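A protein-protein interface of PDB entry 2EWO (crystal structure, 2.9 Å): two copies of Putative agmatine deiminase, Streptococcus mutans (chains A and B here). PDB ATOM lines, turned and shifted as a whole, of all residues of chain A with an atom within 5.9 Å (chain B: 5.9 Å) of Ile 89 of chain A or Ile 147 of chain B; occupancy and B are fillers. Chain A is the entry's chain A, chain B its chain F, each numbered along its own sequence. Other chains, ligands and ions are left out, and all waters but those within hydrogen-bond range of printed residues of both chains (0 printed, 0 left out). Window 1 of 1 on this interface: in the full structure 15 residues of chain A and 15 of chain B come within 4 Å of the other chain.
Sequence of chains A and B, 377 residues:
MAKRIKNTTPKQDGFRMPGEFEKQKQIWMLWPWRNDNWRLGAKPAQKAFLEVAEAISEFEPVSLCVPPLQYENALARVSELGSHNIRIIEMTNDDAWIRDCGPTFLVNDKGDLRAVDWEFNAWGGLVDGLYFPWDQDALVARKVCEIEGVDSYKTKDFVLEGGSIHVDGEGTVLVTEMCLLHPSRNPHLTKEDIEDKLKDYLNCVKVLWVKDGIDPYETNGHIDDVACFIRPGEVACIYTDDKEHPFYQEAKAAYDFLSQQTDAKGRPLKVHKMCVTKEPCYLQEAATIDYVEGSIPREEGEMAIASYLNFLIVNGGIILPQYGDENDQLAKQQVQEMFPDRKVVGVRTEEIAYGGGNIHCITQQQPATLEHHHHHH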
ATOM      1  N   TRP A  28      18.224   1.534  31.375  1.00  0.00           N
ATOM      2  CA  TRP A  28      17.390   0.382  31.088  1.00  0.00           C
ATOM      3  C   TRP A  28      16.050   0.816  30.520  1.00  0.00           C
ATOM      4  O   TRP A  28      15.474   1.804  30.975  1.00  0.00           O
ATOM      5  CB  TRP A  28      17.130  -0.416  32.370  1.00  0.00           C
ATOM      6  CG  TRP A  28      18.363  -1.008  32.995  1.00  0.00           C
ATOM      7  CD1 TRP A  28      19.218  -0.404  33.884  1.00  0.00           C
ATOM      8  CD2 TRP A  28      18.879  -2.325  32.779  1.00  0.00           C
ATOM      9  NE1 TRP A  28      20.230  -1.266  34.233  1.00  0.00           N
ATOM     10  CE2 TRP A  28      20.046  -2.450  33.567  1.00  0.00           C
ATOM     11  CE3 TRP A  28      18.467  -3.414  31.994  1.00  0.00           C
ATOM     12  CZ2 TRP A  28      20.804  -3.611  33.592  1.00  0.00           C
ATOM     13  CZ3 TRP A  28      19.222  -4.568  32.022  1.00  0.00           C
ATOM     14  CH2 TRP A  28      20.379  -4.656  32.817  1.00  0.00           C
ATOM     15  N   SER A  63      20.486  -0.596  27.775  1.00  0.00           N
ATOM     16  CA  SER A  63      20.120  -2.002  28.011  1.00  0.00           C
ATOM     17  C   SER A  63      18.661  -2.163  27.634  1.00  0.00           C
ATOM     18  O   SER A  63      17.769  -1.983  28.450  1.00  0.00           O
ATOM     19  CB  SER A  63      20.311  -2.372  29.482  1.00  0.00           C
ATOM     20  OG  SER A  63      21.690  -2.533  29.778  1.00  0.00           O
ATOM     21  N   LEU A  64      18.445  -2.503  26.375  1.00  0.00           N
ATOM     22  CA  LEU A  64      17.125  -2.687  25.804  1.00  0.00           C
ATOM     23  C   LEU A  64      16.607  -4.117  26.058  1.00  0.00           C
ATOM     24  O   LEU A  64      17.107  -5.071  25.463  1.00  0.00           O
ATOM     25  CB  LEU A  64      17.236  -2.408  24.306  1.00  0.00           C
ATOM     26  CG  LEU A  64      15.962  -2.220  23.506  1.00  0.00           C
ATOM     27  CD1 LEU A  64      15.260  -0.983  24.030  1.00  0.00           C
ATOM     28  CD2 LEU A  64      16.273  -2.102  22.033  1.00  0.00           C
ATOM     29  N   CYS A  65      15.608  -4.271  26.926  1.00  0.00           N
ATOM     30  CA  CYS A  65      15.078  -5.604  27.235  1.00  0.00           C
ATOM     31  C   CYS A  65      13.806  -5.938  26.482  1.00  0.00           C
ATOM     32  O   CYS A  65      12.755  -5.378  26.773  1.00  0.00           O
ATOM     33  CB  CYS A  65      14.791  -5.705  28.722  1.00  0.00           C
ATOM     34  SG  CYS A  65      16.080  -4.979  29.696  1.00  0.00           S
ATOM     35  N   VAL A  66      13.864  -6.861  25.532  1.00  0.00           N
ATOM     36  CA  VAL A  66      12.636  -7.152  24.811  1.00  0.00           C
ATOM     37  C   VAL A  66      12.129  -8.585  24.951  1.00  0.00           C
ATOM     38  O   VAL A  66      12.912  -9.536  25.100  1.00  0.00           O
ATOM     39  CB  VAL A  66      12.763  -6.775  23.296  1.00  0.00           C
ATOM     40  CG1 VAL A  66      13.581  -5.507  23.159  1.00  0.00           C
ATOM     41  CG2 VAL A  66      13.379  -7.908  22.491  1.00  0.00           C
ATOM     42  N   PRO A  67      10.795  -8.745  24.968  1.00  0.00           N
ATOM     43  CA  PRO A  67      10.185 -10.060  25.085  1.00  0.00           C
ATOM     44  C   PRO A  67      10.765 -10.912  23.988  1.00  0.00           C
ATOM     45  O   PRO A  67      11.139 -10.391  22.949  1.00  0.00           O
ATOM     46  CB  PRO A  67       8.707  -9.761  24.876  1.00  0.00           C
ATOM     47  CG  PRO A  67       8.556  -8.482  25.612  1.00  0.00           C
ATOM     48  CD  PRO A  67       9.777  -7.695  25.158  1.00  0.00           C
ATOM     49  N   TYR A  71      12.387 -10.266  19.800  1.00  0.00           N
ATOM     50  CA  TYR A  71      13.819 -10.128  20.056  1.00  0.00           C
ATOM     51  C   TYR A  71      14.594  -9.978  18.752  1.00  0.00           C
ATOM     52  O   TYR A  71      15.216  -8.947  18.510  1.00  0.00           O
ATOM     53  CB  TYR A  71      14.324 -11.335  20.839  1.00  0.00           C
ATOM     54  CG  TYR A  71      15.767 -11.239  21.276  1.00  0.00           C
ATOM     55  CD1 TYR A  71      16.806 -11.661  20.450  1.00  0.00           C
ATOM     56  CD2 TYR A  71      16.094 -10.754  22.536  1.00  0.00           C
ATOM     57  CE1 TYR A  71      18.139 -11.610  20.883  1.00  0.00           C
ATOM     58  CE2 TYR A  71      17.418 -10.703  22.966  1.00  0.00           C
ATOM     59  CZ  TYR A  71      18.423 -11.135  22.142  1.00  0.00           C
ATOM     60  OH  TYR A  71      19.706 -11.143  22.614  1.00  0.00           O
ATOM     61  N   ARG A  87      22.768  -2.877  24.014  1.00  0.00           N
ATOM     62  CA  ARG A  87      22.665  -4.340  24.089  1.00  0.00           C
ATOM     63  C   ARG A  87      21.218  -4.772  24.267  1.00  0.00           C
ATOM     64  O   ARG A  87      20.471  -4.196  25.062  1.00  0.00           O
ATOM     65  CB  ARG A  87      23.499  -4.911  25.243  1.00  0.00           C
ATOM     66  CG  ARG A  87      23.020  -4.554  26.643  1.00  0.00           C
ATOM     67  CD  ARG A  87      23.821  -5.333  27.677  1.00  0.00           C
ATOM     68  NE  ARG A  87      23.481  -4.977  29.054  1.00  0.00           N
ATOM     69  CZ  ARG A  87      24.039  -5.539  30.122  1.00  0.00           C
ATOM     70  NH1 ARG A  87      24.957  -6.479  29.965  1.00  0.00           N
ATOM     71  NH2 ARG A  87      23.686  -5.163  31.344  1.00  0.00           N
ATOM     72  N   ILE A  88      20.829  -5.795  23.521  1.00  0.00           N
ATOM     73  CA  ILE A  88      19.474  -6.310  23.600  1.00  0.00           C
ATOM     74  C   ILE A  88      19.444  -7.567  24.465  1.00  0.00           C
ATOM     75  O   ILE A  88      19.963  -8.606  24.059  1.00  0.00           O
ATOM     76  CB  ILE A  88      18.927  -6.677  22.205  1.00  0.00           C
ATOM     77  CG1 ILE A  88      18.905  -5.446  21.286  1.00  0.00           C
ATOM     78  CG2 ILE A  88      17.535  -7.216  22.342  1.00  0.00           C
ATOM     79  CD1 ILE A  88      20.275  -5.001  20.779  1.00  0.00           C
ATOM     80  N   ILE A  89      18.868  -7.471  25.664  1.00  0.00           N
ATOM     81  CA  ILE A  89      18.758  -8.640  26.547  1.00  0.00           C
ATOM     82  C   ILE A  89      17.322  -9.138  26.517  1.00  0.00           C
ATOM     83  O   ILE A  89      16.384  -8.343  26.482  1.00  0.00           O
ATOM     84  CB  ILE A  89      19.138  -8.346  28.042  1.00  0.00           C
ATOM     85  CG1 ILE A  89      18.324  -7.176  28.589  1.00  0.00           C
ATOM     86  CG2 ILE A  89      20.633  -8.070  28.166  1.00  0.00           C
ATOM     87  CD1 ILE A  89      18.716  -5.831  28.000  1.00  0.00           C
ATOM     88  N   GLU A  90      17.145 -10.454  26.523  1.00  0.00           N
ATOM     89  CA  GLU A  90      15.806 -11.025  26.492  1.00  0.00           C
ATOM     90  C   GLU A  90      15.085 -10.862  27.820  1.00  0.00           C
ATOM     91  O   GLU A  90      15.598 -11.286  28.857  1.00  0.00           O
ATOM     92  CB  GLU A  90      15.871 -12.504  26.171  1.00  0.00           C
ATOM     93  CG  GLU A  90      14.513 -13.063  25.882  1.00  0.00           C
ATOM     94  CD  GLU A  90      14.417 -14.512  26.242  1.00  0.00           C
ATOM     95  OE1 GLU A  90      15.203 -15.305  25.690  1.00  0.00           O
ATOM     96  OE2 GLU A  90      13.561 -14.852  27.083  1.00  0.00           O
ATOM     97  N   MET A  91      13.898 -10.261  27.790  1.00  0.00           N
ATOM     98  CA  MET A  91      13.116 -10.083  29.007  1.00  0.00           C
ATOM     99  C   MET A  91      11.632  -9.907  28.717  1.00  0.00           C
ATOM    100  O   MET A  91      11.266  -9.077  27.895  1.00  0.00           O
ATOM    101  CB  MET A  91      13.622  -8.879  29.787  1.00  0.00           C
ATOM    102  CG  MET A  91      13.083  -8.817  31.186  1.00  0.00           C
ATOM    103  SD  MET A  91      13.924  -7.459  32.294  1.00  0.00           S
ATOM    104  CE  MET A  91      15.795  -7.846  31.959  1.00  0.00           C
ATOM    105  N   ILE A 147      20.914  -9.988  36.444  1.00  0.00           N
ATOM    106  CA  ILE A 147      21.923  -9.933  35.403  1.00  0.00           C
ATOM    107  C   ILE A 147      22.856  -8.772  35.612  1.00  0.00           C
ATOM    108  O   ILE A 147      23.629  -8.434  34.726  1.00  0.00           O
ATOM    109  CB  ILE A 147      21.299  -9.786  34.007  1.00  0.00           C
ATOM    110  CG1 ILE A 147      20.902  -8.338  33.756  1.00  0.00           C
ATOM    111  CG2 ILE A 147      20.060 -10.650  33.909  1.00  0.00           C
ATOM    112  CD1 ILE A 147      20.378  -8.119  32.361  1.00  0.00           C
ATOM    113  N   ALA B   2      27.962  -5.034  20.793  1.00  0.00           N
ATOM    114  CA  ALA B   2      27.626  -6.458  20.494  1.00  0.00           C
ATOM    115  C   ALA B   2      27.260  -6.606  19.019  1.00  0.00           C
ATOM    116  O   ALA B   2      26.141  -6.995  18.684  1.00  0.00           O
ATOM    117  CB  ALA B   2      26.470  -6.921  21.388  1.00  0.00           C
ATOM    118  N   TRP B  28      28.749 -20.865  31.266  1.00  0.00           N
ATOM    119  CA  TRP B  28      27.372 -20.747  30.823  1.00  0.00           C
ATOM    120  C   TRP B  28      26.722 -22.117  30.723  1.00  0.00           C
ATOM    121  O   TRP B  28      27.357 -23.074  30.279  1.00  0.00           O
ATOM    122  CB  TRP B  28      27.316 -20.088  29.441  1.00  0.00           C
ATOM    123  CG  TRP B  28      27.830 -18.675  29.404  1.00  0.00           C
ATOM    124  CD1 TRP B  28      29.130 -18.267  29.232  1.00  0.00           C
ATOM    125  CD2 TRP B  28      27.051 -17.484  29.544  1.00  0.00           C
ATOM    126  NE1 TRP B  28      29.202 -16.894  29.253  1.00  0.00           N
ATOM    127  CE2 TRP B  28      27.943 -16.390  29.446  1.00  0.00           C
ATOM    128  CE3 TRP B  28      25.685 -17.231  29.742  1.00  0.00           C
ATOM    129  CZ2 TRP B  28      27.517 -15.073  29.542  1.00  0.00           C
ATOM    130  CZ3 TRP B  28      25.264 -15.921  29.836  1.00  0.00           C
ATOM    131  CH2 TRP B  28      26.179 -14.859  29.735  1.00  0.00           C
ATOM    132  N   ARG B  87      24.261 -16.486  38.681  1.00  0.00           N
ATOM    133  CA  ARG B  87      23.213 -15.562  38.233  1.00  0.00           C
ATOM    134  C   ARG B  87      22.268 -16.246  37.258  1.00  0.00           C
ATOM    135  O   ARG B  87      22.694 -16.966  36.350  1.00  0.00           O
ATOM    136  CB  ARG B  87      23.804 -14.316  37.558  1.00  0.00           C
ATOM    137  CG  ARG B  87      24.512 -14.555  36.233  1.00  0.00           C
ATOM    138  CD  ARG B  87      24.877 -13.222  35.596  1.00  0.00           C
ATOM    139  NE  ARG B  87      25.642 -13.369  34.358  1.00  0.00           N
ATOM    140  CZ  ARG B  87      26.057 -12.343  33.621  1.00  0.00           C
ATOM    141  NH1 ARG B  87      25.779 -11.106  33.997  1.00  0.00           N
ATOM    142  NH2 ARG B  87      26.754 -12.549  32.509  1.00  0.00           N
ATOM    143  N   ILE B  89      19.873 -15.753  34.295  1.00  0.00           N
ATOM    144  CA  ILE B  89      19.430 -14.835  33.238  1.00  0.00           C
ATOM    145  C   ILE B  89      18.341 -15.517  32.426  1.00  0.00           C
ATOM    146  O   ILE B  89      18.413 -16.718  32.164  1.00  0.00           O
ATOM    147  CB  ILE B  89      20.573 -14.406  32.248  1.00  0.00           C
ATOM    148  CG1 ILE B  89      21.261 -15.631  31.650  1.00  0.00           C
ATOM    149  CG2 ILE B  89      21.583 -13.510  32.960  1.00  0.00           C
ATOM    150  CD1 ILE B  89      22.115 -16.397  32.646  1.00  0.00           C
ATOM    151  N   MET B  91      16.456 -16.865  29.386  1.00  0.00           N
ATOM    152  CA  MET B  91      16.794 -17.241  28.019  1.00  0.00           C
ATOM    153  C   MET B  91      16.025 -18.471  27.555  1.00  0.00           C
ATOM    154  O   MET B  91      16.020 -19.482  28.245  1.00  0.00           O
ATOM    155  CB  MET B  91      18.286 -17.504  27.898  1.00  0.00           C
ATOM    156  CG  MET B  91      18.755 -17.588  26.474  1.00  0.00           C
ATOM    157  SD  MET B  91      20.688 -17.641  26.285  1.00  0.00           S
ATOM    158  CE  MET B  91      21.192 -16.148  27.417  1.00  0.00           C
ATOM    159  N   ARG B 142      23.806 -16.140  19.732  1.00  0.00           N
ATOM    160  CA  ARG B 142      23.752 -14.705  19.473  1.00  0.00           C
ATOM    161  C   ARG B 142      23.316 -13.965  20.735  1.00  0.00           C
ATOM    162  O   ARG B 142      23.911 -12.956  21.106  1.00  0.00           O
ATOM    163  CB  ARG B 142      22.759 -14.414  18.348  1.00  0.00           C
ATOM    164  CG  ARG B 142      22.693 -12.961  17.907  1.00  0.00           C
ATOM    165  CD  ARG B 142      23.845 -12.626  16.986  1.00  0.00           C
ATOM    166  NE  ARG B 142      23.930 -11.209  16.645  1.00  0.00           N
ATOM    167  CZ  ARG B 142      24.494 -10.275  17.411  1.00  0.00           C
ATOM    168  NH1 ARG B 142      25.028 -10.600  18.578  1.00  0.00           N
ATOM    169  NH2 ARG B 142      24.549  -9.015  16.997  1.00  0.00           N
ATOM    170  N   LYS B 143      22.277 -14.478  21.387  1.00  0.00           N
ATOM    171  CA  LYS B 143      21.749 -13.864  22.609  1.00  0.00           C
ATOM    172  C   LYS B 143      22.788 -13.730  23.729  1.00  0.00           C
ATOM    173  O   LYS B 143      22.886 -12.694  24.393  1.00  0.00           O
ATOM    174  CB  LYS B 143      20.560 -14.667  23.150  1.00  0.00           C
ATOM    175  CG  LYS B 143      19.218 -14.497  22.436  1.00  0.00           C
ATOM    176  CD  LYS B 143      18.145 -15.327  23.170  1.00  0.00           C
ATOM    177  CE  LYS B 143      16.817 -15.445  22.417  1.00  0.00           C
ATOM    178  NZ  LYS B 143      15.865 -16.403  23.067  1.00  0.00           N
ATOM    179  N   VAL B 144      23.549 -14.788  23.956  1.00  0.00           N
ATOM    180  CA  VAL B 144      24.555 -14.758  25.000  1.00  0.00           C
ATOM    181  C   VAL B 144      25.720 -13.816  24.640  1.00  0.00           C
ATOM    182  O   VAL B 144      26.358 -13.250  25.523  1.00  0.00           O
ATOM    183  CB  VAL B 144      25.050 -16.189  25.297  1.00  0.00           C
ATOM    184  CG1 VAL B 144      25.595 -16.791  24.037  1.00  0.00           C
ATOM    185  CG2 VAL B 144      26.100 -16.173  26.394  1.00  0.00           C
ATOM    186  N   CYS B 145      26.008 -13.635  23.358  1.00  0.00           N
ATOM    187  CA  CYS B 145      27.069 -12.706  23.010  1.00  0.00           C
ATOM    188  C   CYS B 145      26.559 -11.285  23.201  1.00  0.00           C
ATOM    189  O   CYS B 145      27.346 -10.353  23.286  1.00  0.00           O
ATOM    190  CB  CYS B 145      27.503 -12.841  21.550  1.00  0.00           C
ATOM    191  SG  CYS B 145      28.559 -14.229  21.166  1.00  0.00           S
ATOM    192  N   GLU B 146      25.246 -11.106  23.260  1.00  0.00           N
ATOM    193  CA  GLU B 146      24.701  -9.760  23.396  1.00  0.00           C
ATOM    194  C   GLU B 146      24.808  -9.203  24.785  1.00  0.00           C
ATOM    195  O   GLU B 146      25.158  -8.036  24.965  1.00  0.00           O
ATOM    196  CB  GLU B 146      23.233  -9.727  22.982  1.00  0.00           C
ATOM    197  CG  GLU B 146      22.989  -9.415  21.519  1.00  0.00           C
ATOM    198  CD  GLU B 146      23.392  -7.990  21.124  1.00  0.00           C
ATOM    199  OE1 GLU B 146      22.945  -7.020  21.781  1.00  0.00           O
ATOM    200  OE2 GLU B 146      24.146  -7.842  20.133  1.00  0.00           O
ATOM    201  N   ILE B 147      24.486 -10.039  25.763  1.00  0.00           N
ATOM    202  CA  ILE B 147      24.514  -9.617  27.152  1.00  0.00           C
ATOM    203  C   ILE B 147      25.908  -9.689  27.710  1.00  0.00           C
ATOM    204  O   ILE B 147      26.095  -9.585  28.916  1.00  0.00           O
ATOM    205  CB  ILE B 147      23.611 -10.489  28.034  1.00  0.00           C
ATOM    206  CG1 ILE B 147      24.308 -11.799  28.375  1.00  0.00           C
ATOM    207  CG2 ILE B 147      22.326 -10.805  27.296  1.00  0.00           C
ATOM    208  CD1 ILE B 147      23.506 -12.649  29.324  1.00  0.00           C
ATOM    209  N   GLU B 148      26.892  -9.864  26.839  1.00  0.00           N
ATOM    210  CA  GLU B 148      28.264  -9.952  27.306  1.00  0.00           C
ATOM    211  C   GLU B 148      29.140  -8.909  26.627  1.00  0.00           C
ATOM    212  O   GLU B 148      30.293  -8.712  27.012  1.00  0.00           O
ATOM    213  CB  GLU B 148      28.812 -11.357  27.052  1.00  0.00           C
ATOM    214  CG  GLU B 148      30.079 -11.697  27.831  1.00  0.00           C
ATOM    215  CD  GLU B 148      29.891 -11.653  29.346  1.00  0.00           C
ATOM    216  OE1 GLU B 148      28.799 -12.033  29.830  1.00  0.00           O
ATOM    217  OE2 GLU B 148      30.849 -11.251  30.050  1.00  0.00           O
ATOM    218  N   GLY B 149      28.582  -8.241  25.623  1.00  0.00           N
ATOM    219  CA  GLY B 149      29.318  -7.217  24.910  1.00  0.00           C
ATOM    220  C   GLY B 149      30.495  -7.781  24.153  1.00  0.00           C
ATOM    221  O   GLY B 149      31.626  -7.329  24.325  1.00  0.00           O
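O of Ile 147 of chain B lies within hydrogen-bond range of NH1 of Arg 87 of chain A (3.5 Å).
The backbone NH of Ile 88 of chain A lies within hydrogen-bond range of the side-chain carboxylate of Glu 146 of chain B (3.0 Å).
The side-chain amino group (NZ) of Lys 143 of chain B lies within salt-bridge range of the side-chain carboxylate (OE1) of Glu 90 of chain A (2.9 Å).
OG of Ser 63 of chain A lies within hydrogen-bond range of NE of Arg 87 of chain A.
The backbone carbonyl oxygen of Arg 87 of chain A sits at hydrogen-bond distance from the backbone NH of Leu 64 of chain A, 2.9 Å away.
The backbone NH of Ile 89 of chain A lies within hydrogen-bond range of the backbone carbonyl oxygen of Leu 64 of chain A (3.0 Å).
O of Ile 88 of chain A sits at hydrogen-bond distance from OH of Tyr 71 of chain A (2.9 Å).
The guanidinium group (NH2) of Arg 87 of chain B lies within salt-bridge range of the side-chain carboxylate (OE1) of Glu 148 of chain B.
NH1 of Arg 142 of chain B lies within salt-bridge range of OE2 of Glu 146 of chain B.
Tyr 71 of chain A touches Lys 143 of chain B.
OH of Tyr 71 of chain A touches CB of Glu 146 of chain B, at 3.8 Å.
Arg 87 of chain A touches Glu 146 of chain B (CA to OE1, 3.5 Å).
Ile 147 of chain B touches Ile 89 of chain A (CG2 to CG2, 3.3 Å).
OE1 of Glu 90 of chain A touches CA of Met 91 of chain B (3.4 Å).
NH1 of Arg 87 of chain B touches O of Ile 147 of chain A, 3.5 Å away.
CG2 of Ile 89 of chain B touches CG2 of Ile 147 of chain A (3.4 Å).
Of the printed residues of chain B, Ile 88 of chain A touches Glu 146.
Ile 89 of chain A touches one residue of chain B.
Of the printed residues of chain B, Glu 90 of chain A touches Met 91 (3.4 Å) and Lys 143 (2.9 Å).
Printed residues of chain B within 4 Å of Ile 147 of chain A: Arg 87 (3.5 Å) and Ile 89 (3.4 Å).
Ala 2 of chain B touches none of the printed residues of chain A.
Of the printed residues of chain A, Lys 143 of chain B touches Tyr 71 (3.4 Å) and Glu 90 (2.9 Å).
Of chain A, only Arg 87 (3.5 Å) and Ile 89 (3.3 Å) come within 4 Å of Ile 147 of chain B.
The nearest residue of chain A that does not touch Ile 147 of chain B is Ile 88 of chain A (4.6 Å).
The nearest printed residue of chain B that does not touch Arg 87 of chain A is Glu 148 of chain B (5.0 Å).
Hydrophobic or aromatic side chains of chain A that line the printed part of chain B: Tyr 71, Ile 88, Ile 89 and Ile 147.
Among the printed residues, 10 pairs touch across the chains.
Among the printed residues, Asp or Glu carboxylates within 4 Å of a Lys or Arg side-chain nitrogen of the other chain: Glu 90 of chain A with Lys 143 of chain B (2.9 Å).
Arg 87 of chain A touches Ile 147 of chain B, and with the chains exchanged Ile 147 of chain A touches Arg 87 of chain B.
Ile 89 of chain A touches Ile 147 of chain B, and with the chains exchanged Ile 147 of chain A touches Ile 89 of chain B.
5 positions are printed for both chains.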
